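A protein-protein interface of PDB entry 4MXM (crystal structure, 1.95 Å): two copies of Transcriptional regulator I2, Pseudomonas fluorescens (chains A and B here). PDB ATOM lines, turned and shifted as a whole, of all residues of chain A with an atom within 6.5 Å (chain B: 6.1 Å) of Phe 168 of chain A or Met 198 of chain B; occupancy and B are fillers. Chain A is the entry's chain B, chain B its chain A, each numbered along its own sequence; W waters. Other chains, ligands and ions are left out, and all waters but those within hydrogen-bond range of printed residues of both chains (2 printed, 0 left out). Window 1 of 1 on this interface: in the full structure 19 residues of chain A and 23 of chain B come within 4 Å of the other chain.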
ATOM      1  N   ARG A 159      -4.708  22.347 -16.407  1.00  0.00           N
ATOM      2  CA  ARG A 159      -5.264  23.693 -16.390  1.00  0.00           C
ATOM      3  C   ARG A 159      -6.673  23.752 -16.976  1.00  0.00           C
ATOM      4  O   ARG A 159      -7.423  24.691 -16.709  1.00  0.00           O
ATOM      5  CB  ARG A 159      -4.329  24.661 -17.116  1.00  0.00           C
ATOM      6  CG  ARG A 159      -3.843  24.171 -18.469  1.00  0.00           C
ATOM      7  CD  ARG A 159      -2.447  24.699 -18.752  1.00  0.00           C
ATOM      8  NE  ARG A 159      -2.266  25.079 -20.149  1.00  0.00           N
ATOM      9  CZ  ARG A 159      -2.568  26.278 -20.635  1.00  0.00           C
ATOM     10  NH1 ARG A 159      -2.369  26.545 -21.919  1.00  0.00           N
ATOM     11  NH2 ARG A 159      -3.070  27.209 -19.837  1.00  0.00           N
ATOM     12  N   GLY A 160      -7.033  22.746 -17.764  1.00  0.00           N
ATOM     13  CA  GLY A 160      -8.348  22.701 -18.377  1.00  0.00           C
ATOM     14  C   GLY A 160      -9.372  21.930 -17.563  1.00  0.00           C
ATOM     15  O   GLY A 160      -9.082  21.451 -16.466  1.00  0.00           O
ATOM     16  N   PHE A 163     -13.246  16.726 -17.420  1.00  0.00           N
ATOM     17  CA  PHE A 163     -14.035  15.894 -18.322  1.00  0.00           C
ATOM     18  C   PHE A 163     -13.637  16.112 -19.779  1.00  0.00           C
ATOM     19  O   PHE A 163     -13.532  15.158 -20.546  1.00  0.00           O
ATOM     20  CB  PHE A 163     -15.528  16.170 -18.139  1.00  0.00           C
ATOM     21  CG  PHE A 163     -16.045  15.827 -16.772  1.00  0.00           C
ATOM     22  CD1 PHE A 163     -16.523  14.556 -16.498  1.00  0.00           C
ATOM     23  CD2 PHE A 163     -16.053  16.773 -15.762  1.00  0.00           C
ATOM     24  CE1 PHE A 163     -17.002  14.237 -15.241  1.00  0.00           C
ATOM     25  CE2 PHE A 163     -16.529  16.460 -14.503  1.00  0.00           C
ATOM     26  CZ  PHE A 163     -17.003  15.190 -14.243  1.00  0.00           C
ATOM     27  N   ILE A 164     -13.411  17.370 -20.148  1.00  0.00           N
ATOM     28  CA  ILE A 164     -12.992  17.722 -21.503  1.00  0.00           C
ATOM     29  C   ILE A 164     -11.566  17.248 -21.787  1.00  0.00           C
ATOM     30  O   ILE A 164     -11.255  16.840 -22.909  1.00  0.00           O
ATOM     31  CB  ILE A 164     -13.142  19.244 -21.761  1.00  0.00           C
ATOM     32  CG1 ILE A 164     -14.623  19.620 -21.761  1.00  0.00           C
ATOM     33  CG2 ILE A 164     -12.527  19.658 -23.087  1.00  0.00           C
ATOM     34  CD1 ILE A 164     -14.897  21.036 -22.232  1.00  0.00           C
ATOM     35  N   THR A 165     -10.709  17.295 -20.770  1.00  0.00           N
ATOM     36  CA  THR A 165      -9.349  16.775 -20.896  1.00  0.00           C
ATOM     37  C   THR A 165      -9.385  15.280 -21.211  1.00  0.00           C
ATOM     38  O   THR A 165      -8.657  14.801 -22.082  1.00  0.00           O
ATOM     39  CB  THR A 165      -8.529  17.006 -19.612  1.00  0.00           C
ATOM     40  OG1 THR A 165      -8.488  18.407 -19.318  1.00  0.00           O
ATOM     41  CG2 THR A 165      -7.113  16.482 -19.774  1.00  0.00           C
ATOM     42  N   ARG A 166     -10.242  14.550 -20.502  1.00  0.00           N
ATOM     43  CA  ARG A 166     -10.410  13.121 -20.738  1.00  0.00           C
ATOM     44  C   ARG A 166     -10.899  12.835 -22.160  1.00  0.00           C
ATOM     45  O   ARG A 166     -10.388  11.935 -22.826  1.00  0.00           O
ATOM     46  CB  ARG A 166     -11.370  12.519 -19.707  1.00  0.00           C
ATOM     47  CG  ARG A 166     -11.826  11.097 -20.021  1.00  0.00           C
ATOM     48  CD  ARG A 166     -10.657  10.128 -20.135  1.00  0.00           C
ATOM     49  NE  ARG A 166     -11.088   8.814 -20.606  1.00  0.00           N
ATOM     50  CZ  ARG A 166     -10.302   7.955 -21.248  1.00  0.00           C
ATOM     51  NH1 ARG A 166      -9.040   8.270 -21.501  1.00  0.00           N
ATOM     52  NH2 ARG A 166     -10.780   6.782 -21.642  1.00  0.00           N
ATOM     53  N   ARG A 167     -11.884  13.600 -22.621  1.00  0.00           N
ATOM     54  CA  ARG A 167     -12.429  13.402 -23.960  1.00  0.00           C
ATOM     55  C   ARG A 167     -11.393  13.727 -25.037  1.00  0.00           C
ATOM     56  O   ARG A 167     -11.331  13.060 -26.068  1.00  0.00           O
ATOM     57  CB  ARG A 167     -13.709  14.220 -24.153  1.00  0.00           C
ATOM     58  CG  ARG A 167     -14.810  13.859 -23.163  1.00  0.00           C
ATOM     59  CD  ARG A 167     -16.146  14.483 -23.532  1.00  0.00           C
ATOM     60  NE  ARG A 167     -17.166  14.224 -22.519  1.00  0.00           N
ATOM     61  CZ  ARG A 167     -17.627  15.135 -21.668  1.00  0.00           C
ATOM     62  NH1 ARG A 167     -18.553  14.806 -20.779  1.00  0.00           N
ATOM     63  NH2 ARG A 167     -17.168  16.379 -21.711  1.00  0.00           N
ATOM     64  N   PHE A 168     -10.579  14.746 -24.786  1.00  0.00           N
ATOM     65  CA  PHE A 168      -9.458  15.059 -25.667  1.00  0.00           C
ATOM     66  C   PHE A 168      -8.456  13.912 -25.685  1.00  0.00           C
ATOM     67  O   PHE A 168      -7.999  13.485 -26.747  1.00  0.00           O
ATOM     68  CB  PHE A 168      -8.754  16.336 -25.211  1.00  0.00           C
ATOM     69  CG  PHE A 168      -9.454  17.597 -25.617  1.00  0.00           C
ATOM     70  CD1 PHE A 168     -10.282  17.622 -26.727  1.00  0.00           C
ATOM     71  CD2 PHE A 168      -9.276  18.764 -24.894  1.00  0.00           C
ATOM     72  CE1 PHE A 168     -10.925  18.786 -27.103  1.00  0.00           C
ATOM     73  CE2 PHE A 168      -9.912  19.930 -25.268  1.00  0.00           C
ATOM     74  CZ  PHE A 168     -10.740  19.941 -26.372  1.00  0.00           C
ATOM     75  N   LEU A 169      -8.116  13.417 -24.500  1.00  0.00           N
ATOM     76  CA  LEU A 169      -7.130  12.352 -24.369  1.00  0.00           C
ATOM     77  C   LEU A 169      -7.624  11.055 -25.000  1.00  0.00           C
ATOM     78  O   LEU A 169      -6.840  10.293 -25.564  1.00  0.00           O
ATOM     79  CB  LEU A 169      -6.771  12.130 -22.897  1.00  0.00           C
ATOM     80  CG  LEU A 169      -5.562  11.236 -22.621  1.00  0.00           C
ATOM     81  CD1 LEU A 169      -4.391  11.637 -23.504  1.00  0.00           C
ATOM     82  CD2 LEU A 169      -5.171  11.321 -21.158  1.00  0.00           C
ATOM     83  N   THR A 170      -8.930  10.816 -24.911  1.00  0.00           N
ATOM     84  CA  THR A 170      -9.542   9.629 -25.494  1.00  0.00           C
ATOM     85  C   THR A 170      -9.302   9.569 -27.000  1.00  0.00           C
ATOM     86  O   THR A 170      -8.896   8.538 -27.533  1.00  0.00           O
ATOM     87  CB  THR A 170     -11.063   9.599 -25.239  1.00  0.00           C
ATOM     88  OG1 THR A 170     -11.316   9.687 -23.832  1.00  0.00           O
ATOM     89  CG2 THR A 170     -11.673   8.315 -25.780  1.00  0.00           C
ATOM     90  N   GLY A 171      -9.550  10.686 -27.677  1.00  0.00           N
ATOM     91  CA  GLY A 171      -9.379  10.759 -29.115  1.00  0.00           C
ATOM     92  C   GLY A 171      -7.922  10.771 -29.527  1.00  0.00           C
ATOM     93  O   GLY A 171      -7.553  10.198 -30.548  1.00  0.00           O
ATOM     94  N   ALA A 172      -7.091  11.432 -28.726  1.00  0.00           N
ATOM     95  CA  ALA A 172      -5.663  11.504 -28.993  1.00  0.00           C
ATOM     96  C   ALA A 172      -5.024  10.117 -28.975  1.00  0.00           C
ATOM     97  O   ALA A 172      -4.210   9.788 -29.838  1.00  0.00           O
ATOM     98  CB  ALA A 172      -4.984  12.417 -27.986  1.00  0.00           C
ATOM     99  N   LEU A 173      -5.411   9.303 -27.997  1.00  0.00           N
ATOM    100  CA  LEU A 173      -4.838   7.969 -27.835  1.00  0.00           C
ATOM    101  C   LEU A 173      -5.401   6.941 -28.820  1.00  0.00           C
ATOM    102  O   LEU A 173      -4.672   6.075 -29.300  1.00  0.00           O
ATOM    103  CB  LEU A 173      -5.020   7.474 -26.396  1.00  0.00           C
ATOM    104  CG  LEU A 173      -4.313   8.261 -25.289  1.00  0.00           C
ATOM    105  CD1 LEU A 173      -4.515   7.579 -23.941  1.00  0.00           C
ATOM    106  CD2 LEU A 173      -2.828   8.431 -25.593  1.00  0.00           C
ATOM    107  N   LEU A 197       3.622  14.253 -21.500  1.00  0.00           N
ATOM    108  CA  LEU A 197       4.262  15.558 -21.644  1.00  0.00           C
ATOM    109  C   LEU A 197       3.301  16.638 -22.128  1.00  0.00           C
ATOM    110  O   LEU A 197       3.440  17.808 -21.772  1.00  0.00           O
ATOM    111  CB  LEU A 197       5.460  15.467 -22.595  1.00  0.00           C
ATOM    112  CG  LEU A 197       6.720  14.797 -22.047  1.00  0.00           C
ATOM    113  CD1 LEU A 197       7.784  14.680 -23.127  1.00  0.00           C
ATOM    114  CD2 LEU A 197       7.249  15.575 -20.854  1.00  0.00           C
ATOM    115  N   MET A 198       2.328  16.244 -22.941  1.00  0.00           N
ATOM    116  CA  MET A 198       1.365  17.191 -23.487  1.00  0.00           C
ATOM    117  C   MET A 198       0.232  17.489 -22.510  1.00  0.00           C
ATOM    118  O   MET A 198      -0.182  18.637 -22.359  1.00  0.00           O
ATOM    119  CB  MET A 198       0.782  16.667 -24.800  1.00  0.00           C
ATOM    120  CG  MET A 198      -0.226  17.605 -25.441  1.00  0.00           C
ATOM    121  SD  MET A 198      -1.250  16.757 -26.863  1.00  0.00           S
ATOM    122  CE  MET A 198      -2.167  15.398 -25.804  1.00  0.00           C
ATOM    123  N   VAL A 199      -0.263  16.449 -21.844  1.00  0.00           N
ATOM    124  CA  VAL A 199      -1.478  16.570 -21.041  1.00  0.00           C
ATOM    125  C   VAL A 199      -1.247  17.141 -19.637  1.00  0.00           C
ATOM    126  O   VAL A 199      -2.154  17.730 -19.048  1.00  0.00           O
ATOM    127  CB  VAL A 199      -2.240  15.221 -20.961  1.00  0.00           C
ATOM    128  CG1 VAL A 199      -1.635  14.315 -19.897  1.00  0.00           C
ATOM    129  CG2 VAL A 199      -3.716  15.458 -20.690  1.00  0.00           C
ATOM    130  N   LEU A 200      -0.040  16.981 -19.105  1.00  0.00           N
ATOM    131  CA  LEU A 200       0.268  17.491 -17.771  1.00  0.00           C
ATOM    132  C   LEU A 200       1.183  18.709 -17.821  1.00  0.00           C
ATOM    133  O   LEU A 200       2.109  18.767 -18.629  1.00  0.00           O
ATOM    134  CB  LEU A 200       0.894  16.401 -16.896  1.00  0.00           C
ATOM    135  CG  LEU A 200       0.024  15.192 -16.548  1.00  0.00           C
ATOM    136  CD1 LEU A 200       0.630  14.410 -15.388  1.00  0.00           C
ATOM    137  CD2 LEU A 200      -1.399  15.617 -16.228  1.00  0.00           C
ATOM    138  N   PHE B 168      -1.398  13.805 -31.869  1.00  0.00           N
ATOM    139  CA  PHE B 168      -2.283  13.772 -30.707  1.00  0.00           C
ATOM    140  C   PHE B 168      -3.440  14.748 -30.882  1.00  0.00           C
ATOM    141  O   PHE B 168      -4.600  14.398 -30.668  1.00  0.00           O
ATOM    142  CB  PHE B 168      -1.516  14.125 -29.432  1.00  0.00           C
ATOM    143  CG  PHE B 168      -0.655  13.013 -28.910  1.00  0.00           C
ATOM    144  CD1 PHE B 168      -0.957  11.692 -29.191  1.00  0.00           C
ATOM    145  CD2 PHE B 168       0.455  13.291 -28.129  1.00  0.00           C
ATOM    146  CE1 PHE B 168      -0.166  10.669 -28.708  1.00  0.00           C
ATOM    147  CE2 PHE B 168       1.248  12.273 -27.643  1.00  0.00           C
ATOM    148  CZ  PHE B 168       0.939  10.959 -27.932  1.00  0.00           C
ATOM    149  N   LEU B 169      -3.115  15.976 -31.274  1.00  0.00           N
ATOM    150  CA  LEU B 169      -4.118  17.022 -31.427  1.00  0.00           C
ATOM    151  C   LEU B 169      -5.095  16.700 -32.553  1.00  0.00           C
ATOM    152  O   LEU B 169      -6.273  17.047 -32.476  1.00  0.00           O
ATOM    153  CB  LEU B 169      -3.450  18.378 -31.665  1.00  0.00           C
ATOM    154  CG  LEU B 169      -4.347  19.607 -31.526  1.00  0.00           C
ATOM    155  CD1 LEU B 169      -5.003  19.636 -30.152  1.00  0.00           C
ATOM    156  CD2 LEU B 169      -3.547  20.874 -31.761  1.00  0.00           C
ATOM    157  N   GLY B 171      -6.158  13.716 -33.361  1.00  0.00           N
ATOM    158  CA  GLY B 171      -7.097  12.758 -32.811  1.00  0.00           C
ATOM    159  C   GLY B 171      -8.049  13.375 -31.806  1.00  0.00           C
ATOM    160  O   GLY B 171      -9.240  13.063 -31.798  1.00  0.00           O
ATOM    161  N   ALA B 172      -7.522  14.254 -30.959  1.00  0.00           N
ATOM    162  CA  ALA B 172      -8.326  14.911 -29.935  1.00  0.00           C
ATOM    163  C   ALA B 172      -9.439  15.766 -30.539  1.00  0.00           C
ATOM    164  O   ALA B 172     -10.572  15.758 -30.055  1.00  0.00           O
ATOM    165  CB  ALA B 172      -7.440  15.756 -29.030  1.00  0.00           C
ATOM    166  N   LEU B 173      -9.112  16.496 -31.600  1.00  0.00           N
ATOM    167  CA  LEU B 173     -10.070  17.397 -32.233  1.00  0.00           C
ATOM    168  C   LEU B 173     -11.106  16.663 -33.085  1.00  0.00           C
ATOM    169  O   LEU B 173     -12.274  17.042 -33.106  1.00  0.00           O
ATOM    170  CB  LEU B 173      -9.350  18.451 -33.080  1.00  0.00           C
ATOM    171  CG  LEU B 173      -8.415  19.429 -32.363  1.00  0.00           C
ATOM    172  CD1 LEU B 173      -7.891  20.470 -33.343  1.00  0.00           C
ATOM    173  CD2 LEU B 173      -9.106  20.096 -31.183  1.00  0.00           C
ATOM    174  N   TRP B 175     -12.206  13.655 -32.660  1.00  0.00           N
ATOM    175  CA  TRP B 175     -13.076  12.874 -31.783  1.00  0.00           C
ATOM    176  C   TRP B 175     -14.213  13.719 -31.206  1.00  0.00           C
ATOM    177  O   TRP B 175     -15.168  13.188 -30.632  1.00  0.00           O
ATOM    178  CB  TRP B 175     -12.252  12.236 -30.659  1.00  0.00           C
ATOM    179  CG  TRP B 175     -13.038  11.372 -29.717  1.00  0.00           C
ATOM    180  CD1 TRP B 175     -13.338  11.645 -28.413  1.00  0.00           C
ATOM    181  CD2 TRP B 175     -13.623  10.095 -30.004  1.00  0.00           C
ATOM    182  NE1 TRP B 175     -14.071  10.618 -27.870  1.00  0.00           N
ATOM    183  CE2 TRP B 175     -14.261   9.655 -28.826  1.00  0.00           C
ATOM    184  CE3 TRP B 175     -13.669   9.282 -31.141  1.00  0.00           C
ATOM    185  CZ2 TRP B 175     -14.937   8.437 -28.753  1.00  0.00           C
ATOM    186  CZ3 TRP B 175     -14.342   8.074 -31.066  1.00  0.00           C
ATOM    187  CH2 TRP B 175     -14.967   7.664 -29.882  1.00  0.00           C
ATOM    188  N   THR B 176     -14.117  15.035 -31.370  1.00  0.00           N
ATOM    189  CA  THR B 176     -15.131  15.947 -30.846  1.00  0.00           C
ATOM    190  C   THR B 176     -16.502  15.760 -31.499  1.00  0.00           C
ATOM    191  O   THR B 176     -17.513  16.204 -30.959  1.00  0.00           O
ATOM    192  CB  THR B 176     -14.704  17.424 -30.982  1.00  0.00           C
ATOM    193  OG1 THR B 176     -14.444  17.727 -32.358  1.00  0.00           O
ATOM    194  CG2 THR B 176     -13.451  17.695 -30.159  1.00  0.00           C
ATOM    195  N   TRP B 179     -19.042  13.936 -29.116  1.00  0.00           N
ATOM    196  CA  TRP B 179     -19.476  14.451 -27.818  1.00  0.00           C
ATOM    197  C   TRP B 179     -19.829  15.941 -27.760  1.00  0.00           C
ATOM    198  O   TRP B 179     -20.517  16.373 -26.835  1.00  0.00           O
ATOM    199  CB  TRP B 179     -18.444  14.110 -26.734  1.00  0.00           C
ATOM    200  CG  TRP B 179     -17.084  14.720 -26.951  1.00  0.00           C
ATOM    201  CD1 TRP B 179     -16.024  14.151 -27.594  1.00  0.00           C
ATOM    202  CD2 TRP B 179     -16.639  16.009 -26.509  1.00  0.00           C
ATOM    203  NE1 TRP B 179     -14.947  15.007 -27.583  1.00  0.00           N
ATOM    204  CE2 TRP B 179     -15.299  16.154 -26.924  1.00  0.00           C
ATOM    205  CE3 TRP B 179     -17.243  17.054 -25.801  1.00  0.00           C
ATOM    206  CZ2 TRP B 179     -14.556  17.302 -26.657  1.00  0.00           C
ATOM    207  CZ3 TRP B 179     -16.503  18.192 -25.538  1.00  0.00           C
ATOM    208  CH2 TRP B 179     -15.174  18.306 -25.965  1.00  0.00           C
ATOM    209  N   LEU B 191     -14.665  25.566 -26.856  1.00  0.00           N
ATOM    210  CA  LEU B 191     -14.037  24.280 -27.128  1.00  0.00           C
ATOM    211  C   LEU B 191     -12.595  24.470 -27.592  1.00  0.00           C
ATOM    212  O   LEU B 191     -11.699  23.721 -27.197  1.00  0.00           O
ATOM    213  CB  LEU B 191     -14.832  23.518 -28.190  1.00  0.00           C
ATOM    214  CG  LEU B 191     -14.226  22.203 -28.685  1.00  0.00           C
ATOM    215  CD1 LEU B 191     -14.029  21.239 -27.527  1.00  0.00           C
ATOM    216  CD2 LEU B 191     -15.094  21.581 -29.765  1.00  0.00           C
ATOM    217  N   GLU B 193     -10.622  27.025 -26.912  1.00  0.00           N
ATOM    218  CA  GLU B 193      -9.825  27.502 -25.788  1.00  0.00           C
ATOM    219  C   GLU B 193      -9.414  26.355 -24.869  1.00  0.00           C
ATOM    220  O   GLU B 193      -8.319  26.365 -24.304  1.00  0.00           O
ATOM    221  CB  GLU B 193     -10.586  28.567 -24.992  1.00  0.00           C
ATOM    222  CG  GLU B 193     -10.841  29.868 -25.748  1.00  0.00           C
ATOM    223  CD  GLU B 193      -9.617  30.768 -25.823  1.00  0.00           C
ATOM    224  OE1 GLU B 193      -8.524  30.346 -25.388  1.00  0.00           O
ATOM    225  OE2 GLU B 193      -9.753  31.910 -26.312  1.00  0.00           O
ATOM    226  N   GLU B 194     -10.298  25.373 -24.717  1.00  0.00           N
ATOM    227  CA  GLU B 194      -9.993  24.187 -23.921  1.00  0.00           C
ATOM    228  C   GLU B 194      -8.884  23.367 -24.569  1.00  0.00           C
ATOM    229  O   GLU B 194      -7.981  22.882 -23.887  1.00  0.00           O
ATOM    230  CB  GLU B 194     -11.243  23.326 -23.729  1.00  0.00           C
ATOM    231  CG  GLU B 194     -12.167  23.814 -22.626  1.00  0.00           C
ATOM    232  CD  GLU B 194     -11.546  23.684 -21.246  1.00  0.00           C
ATOM    233  OE1 GLU B 194     -10.806  22.704 -21.011  1.00  0.00           O
ATOM    234  OE2 GLU B 194     -11.795  24.564 -20.397  1.00  0.00           O
ATOM    235  N   ALA B 195      -8.956  23.218 -25.889  1.00  0.00           N
ATOM    236  CA  ALA B 195      -7.938  22.486 -26.634  1.00  0.00           C
ATOM    237  C   ALA B 195      -6.586  23.185 -26.531  1.00  0.00           C
ATOM    238  O   ALA B 195      -5.541  22.537 -26.506  1.00  0.00           O
ATOM    239  CB  ALA B 195      -8.353  22.324 -28.089  1.00  0.00           C
ATOM    240  N   LEU B 196      -6.615  24.514 -26.471  1.00  0.00           N
ATOM    241  CA  LEU B 196      -5.405  25.314 -26.332  1.00  0.00           C
ATOM    242  C   LEU B 196      -4.802  25.109 -24.948  1.00  0.00           C
ATOM    243  O   LEU B 196      -3.586  24.960 -24.807  1.00  0.00           O
ATOM    244  CB  LEU B 196      -5.729  26.793 -26.546  1.00  0.00           C
ATOM    245  CG  LEU B 196      -4.529  27.734 -26.664  1.00  0.00           C
ATOM    246  CD1 LEU B 196      -3.801  27.497 -27.978  1.00  0.00           C
ATOM    247  CD2 LEU B 196      -4.962  29.188 -26.542  1.00  0.00           C
ATOM    248  N   LEU B 197      -5.665  25.109 -23.935  1.00  0.00           N
ATOM    249  CA  LEU B 197      -5.272  24.844 -22.553  1.00  0.00           C
ATOM    250  C   LEU B 197      -4.585  23.490 -22.426  1.00  0.00           C
ATOM    251  O   LEU B 197      -3.609  23.340 -21.685  1.00  0.00           O
ATOM    252  CB  LEU B 197      -6.504  24.873 -21.650  1.00  0.00           C
ATOM    253  CG  LEU B 197      -6.671  26.049 -20.693  1.00  0.00           C
ATOM    254  CD1 LEU B 197      -6.211  27.332 -21.340  1.00  0.00           C
ATOM    255  CD2 LEU B 197      -8.122  26.172 -20.252  1.00  0.00           C
ATOM    256  N   MET B 198      -5.098  22.514 -23.166  1.00  0.00           N
ATOM    257  CA  MET B 198      -4.567  21.160 -23.150  1.00  0.00           C
ATOM    258  C   MET B 198      -3.157  21.082 -23.725  1.00  0.00           C
ATOM    259  O   MET B 198      -2.242  20.546 -23.096  1.00  0.00           O
ATOM    260  CB  MET B 198      -5.485  20.249 -23.965  1.00  0.00           C
ATOM    261  CG  MET B 198      -6.228  19.197 -23.161  1.00  0.00           C
ATOM    262  SD  MET B 198      -5.551  17.409 -23.533  1.00  0.00           S
ATOM    263  CE  MET B 198      -5.322  17.560 -25.467  1.00  0.00           C
ATOM    264  N   VAL B 199      -2.992  21.623 -24.927  1.00  0.00           N
ATOM    265  CA  VAL B 199      -1.789  21.398 -25.719  1.00  0.00           C
ATOM    266  C   VAL B 199      -0.666  22.409 -25.443  1.00  0.00           C
ATOM    267  O   VAL B 199       0.502  22.143 -25.741  1.00  0.00           O
ATOM    268  CB  VAL B 199      -2.134  21.360 -27.230  1.00  0.00           C
ATOM    269  CG1 VAL B 199      -2.404  22.755 -27.756  1.00  0.00           C
ATOM    270  CG2 VAL B 199      -1.027  20.691 -28.024  1.00  0.00           C
ATOM    271  N   LEU B 200      -1.008  23.556 -24.861  1.00  0.00           N
ATOM    272  CA  LEU B 200      -0.006  24.578 -24.550  1.00  0.00           C
ATOM    273  C   LEU B 200       0.146  24.805 -23.036  1.00  0.00           C
ATOM    274  O   LEU B 200      -0.717  24.392 -22.251  1.00  0.00           O
ATOM    275  CB  LEU B 200      -0.321  25.897 -25.269  1.00  0.00           C
ATOM    276  CG  LEU B 200      -0.327  25.907 -26.804  1.00  0.00           C
ATOM    277  CD1 LEU B 200      -0.250  27.331 -27.352  1.00  0.00           C
ATOM    278  CD2 LEU B 200       0.788  25.039 -27.383  1.00  0.00           C
ATOM    279  N   LYS B 201       1.241  25.452 -22.634  1.00  0.00           N
ATOM    280  CA  LYS B 201       1.512  25.720 -21.219  1.00  0.00           C
ATOM    281  C   LYS B 201       0.924  27.047 -20.754  1.00  0.00           C
ATOM    282  O   LYS B 201       0.172  27.697 -21.480  1.00  0.00           O
ATOM    283  CB  LYS B 201       3.016  25.766 -20.953  1.00  0.00           C
ATOM    284  CG  LYS B 201       3.783  24.516 -21.316  1.00  0.00           C
ATOM    285  CD  LYS B 201       5.247  24.704 -20.976  1.00  0.00           C
ATOM    286  CE  LYS B 201       6.102  23.590 -21.542  1.00  0.00           C
ATOM    287  NZ  LYS B 201       7.547  23.921 -21.415  1.00  0.00           N
HETATM  288  O   HOH W   1      -0.869  21.296 -20.378  1.00  0.00           O
HETATM  289  O   HOH W   2     -12.088  14.788 -28.214  1.00  0.00           O
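Of the printed residues of chain B, Arg 167 of chain A touches Trp 175 (3.4 Å) and Trp 179 (3.4 Å).
Of chain B, only Ala 172 (3.3 Å), Trp 179 (3.9 Å), Leu 191 (3.7 Å), Glu 194 (3.7 Å), Ala 195 (3.5 Å) and Met 198 (3.5 Å) come within 4 Å of Phe 168 of chain A.
Of the printed residues of chain B, Gly 171 of chain A touches Gly 171, Ala 172 and Trp 175.
Leu 173 of chain A touches none of the printed residues of chain B.
Thr 176 of chain B touches none of the printed residues of chain A.
Printed residues of chain A within 4 Å of Glu 194 of chain B: Gly 160, Ile 164 and Phe 168.
Of chain A, only Phe 168, Met 198 and Val 199 come within 4 Å of Met 198 of chain B.
The nearest residue of chain B that does not touch Phe 168 of chain A is Thr 176 of chain B (4.1 Å).
The nearest residue of chain A that does not touch Met 198 of chain B is Thr 165 of chain A (4.2 Å).
The nearest printed residue of chain A that does not touch Leu 191 of chain B is Ile 164 of chain A (4.9 Å).
Of the 17 printed residues of chain A, 10 touch a printed residue of chain B.
Printed residues of chain B that touch a printed residue of chain A: Phe 168, Gly 171, Ala 172, Trp 175, Trp 179, Leu 191, Glu 194, Ala 195, Leu 196, Leu 197, Met 198, Leu 200 and Lys 201.
Hydrophobic or aromatic side chains of chain B within 4 Å of the printed part of chain A: Phe 168, Ala 172, Trp 175, Trp 179, Leu 191, Ala 195, Leu 197, Met 198 and Leu 200.
Among the printed residues, 25 pairs touch across the chains.
O of Arg 166 of chain A sits at hydrogen-bond distance from OG1 of Thr 170 of chain A, 2.6 Å away.
NE of Arg 159 of chain A sits at hydrogen-bond distance from O of Leu 197 of chain B (2.7 Å).
The guanidinium group (NE) of Arg 159 of chain A sits at hydrogen-bond distance from the backbone carbonyl oxygen (O) of Leu 200 of chain B (2.7 Å).
O of Lys 201 of chain B lies within hydrogen-bond range of NH1 of Arg 159 of chain A.
O of Met 198 of chain A lies close to O of Met 198 of chain B, 2.9 Å away.
Among the printed residues, pairs that only touch across the chains: Arg 159 of chain A with Leu 196 of chain B (3.5 Å), Gly 160 of chain A with Glu 194 of chain B (3.6 Å), Gly 160 of chain A with Leu 197 of chain B (3.95 Å), Ile 164 of chain A with Glu 194 of chain B (3.9 Å), Arg 167 of chain A with Trp 175 of chain B (3.4 Å), Arg 167 of chain A with Trp 179 of chain B (3.4 Å), Phe 168 of chain A with Ala 172 of chain B (3.3 Å), Phe 168 of chain A with Trp 179 of chain B (3.9 Å), Phe 168 of chain A with Leu 191 of chain B (3.7 Å), Phe 168 of chain A with Glu 194 of chain B (3.7 Å), Phe 168 of chain A with Ala 195 of chain B (3.5 Å), Phe 168 of chain A with Met 198 of chain B (3.5 Å), Thr 170 of chain A with Trp 175 of chain B (3.9 Å), Gly 171 of chain A with Gly 171 of chain B (3.4 Å), Gly 171 of chain A with Ala 172 of chain B (3.8 Å), Gly 171 of chain A with Trp 175 of chain B (3.6 Å), Ala 172 of chain A with Phe 168 of chain B (3.4 Å), Ala 172 of chain A with Gly 171 of chain B (3.8 Å), Ala 172 of chain A with Ala 172 of chain B (3.6 Å), Met 198 of chain A with Phe 168 of chain B (3.7 Å) and Val 199 of chain A with Met 198 of chain B (3.9 Å).
Phe 168 of chain A touches Ala 172 of chain B, and with the chains exchanged Ala 172 of chain A touches Phe 168 of chain B.
Phe 168 of chain A touches Met 198 of chain B, and with the chains exchanged Met 198 of chain A touches Phe 168 of chain B.
Gly 171 of chain B touches its own counterpart, Gly 171 of chain A.
Gly 171 of chain A touches Ala 172 of chain B, and with the chains exchanged Ala 172 of chain A touches Gly 171 of chain B.
Of the 25 pairs that touch across the chains among the printed residues, 9 have their exchanged pair printed and touching as well.
Water W2 lies within hydrogen-bond range of the backbone carbonyl oxygen of Ala 172 of chain B (2.6 Å), the backbone carbonyl oxygen of Arg 167 of chain A (2.9 Å) and the indole nitrogen of Trp 179 of chain B (2.9 Å).
Water W1 lies within hydrogen-bond range of O of Met 198 of chain B (3.1 Å) and O of Met 198 of chain A (3.4 Å).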
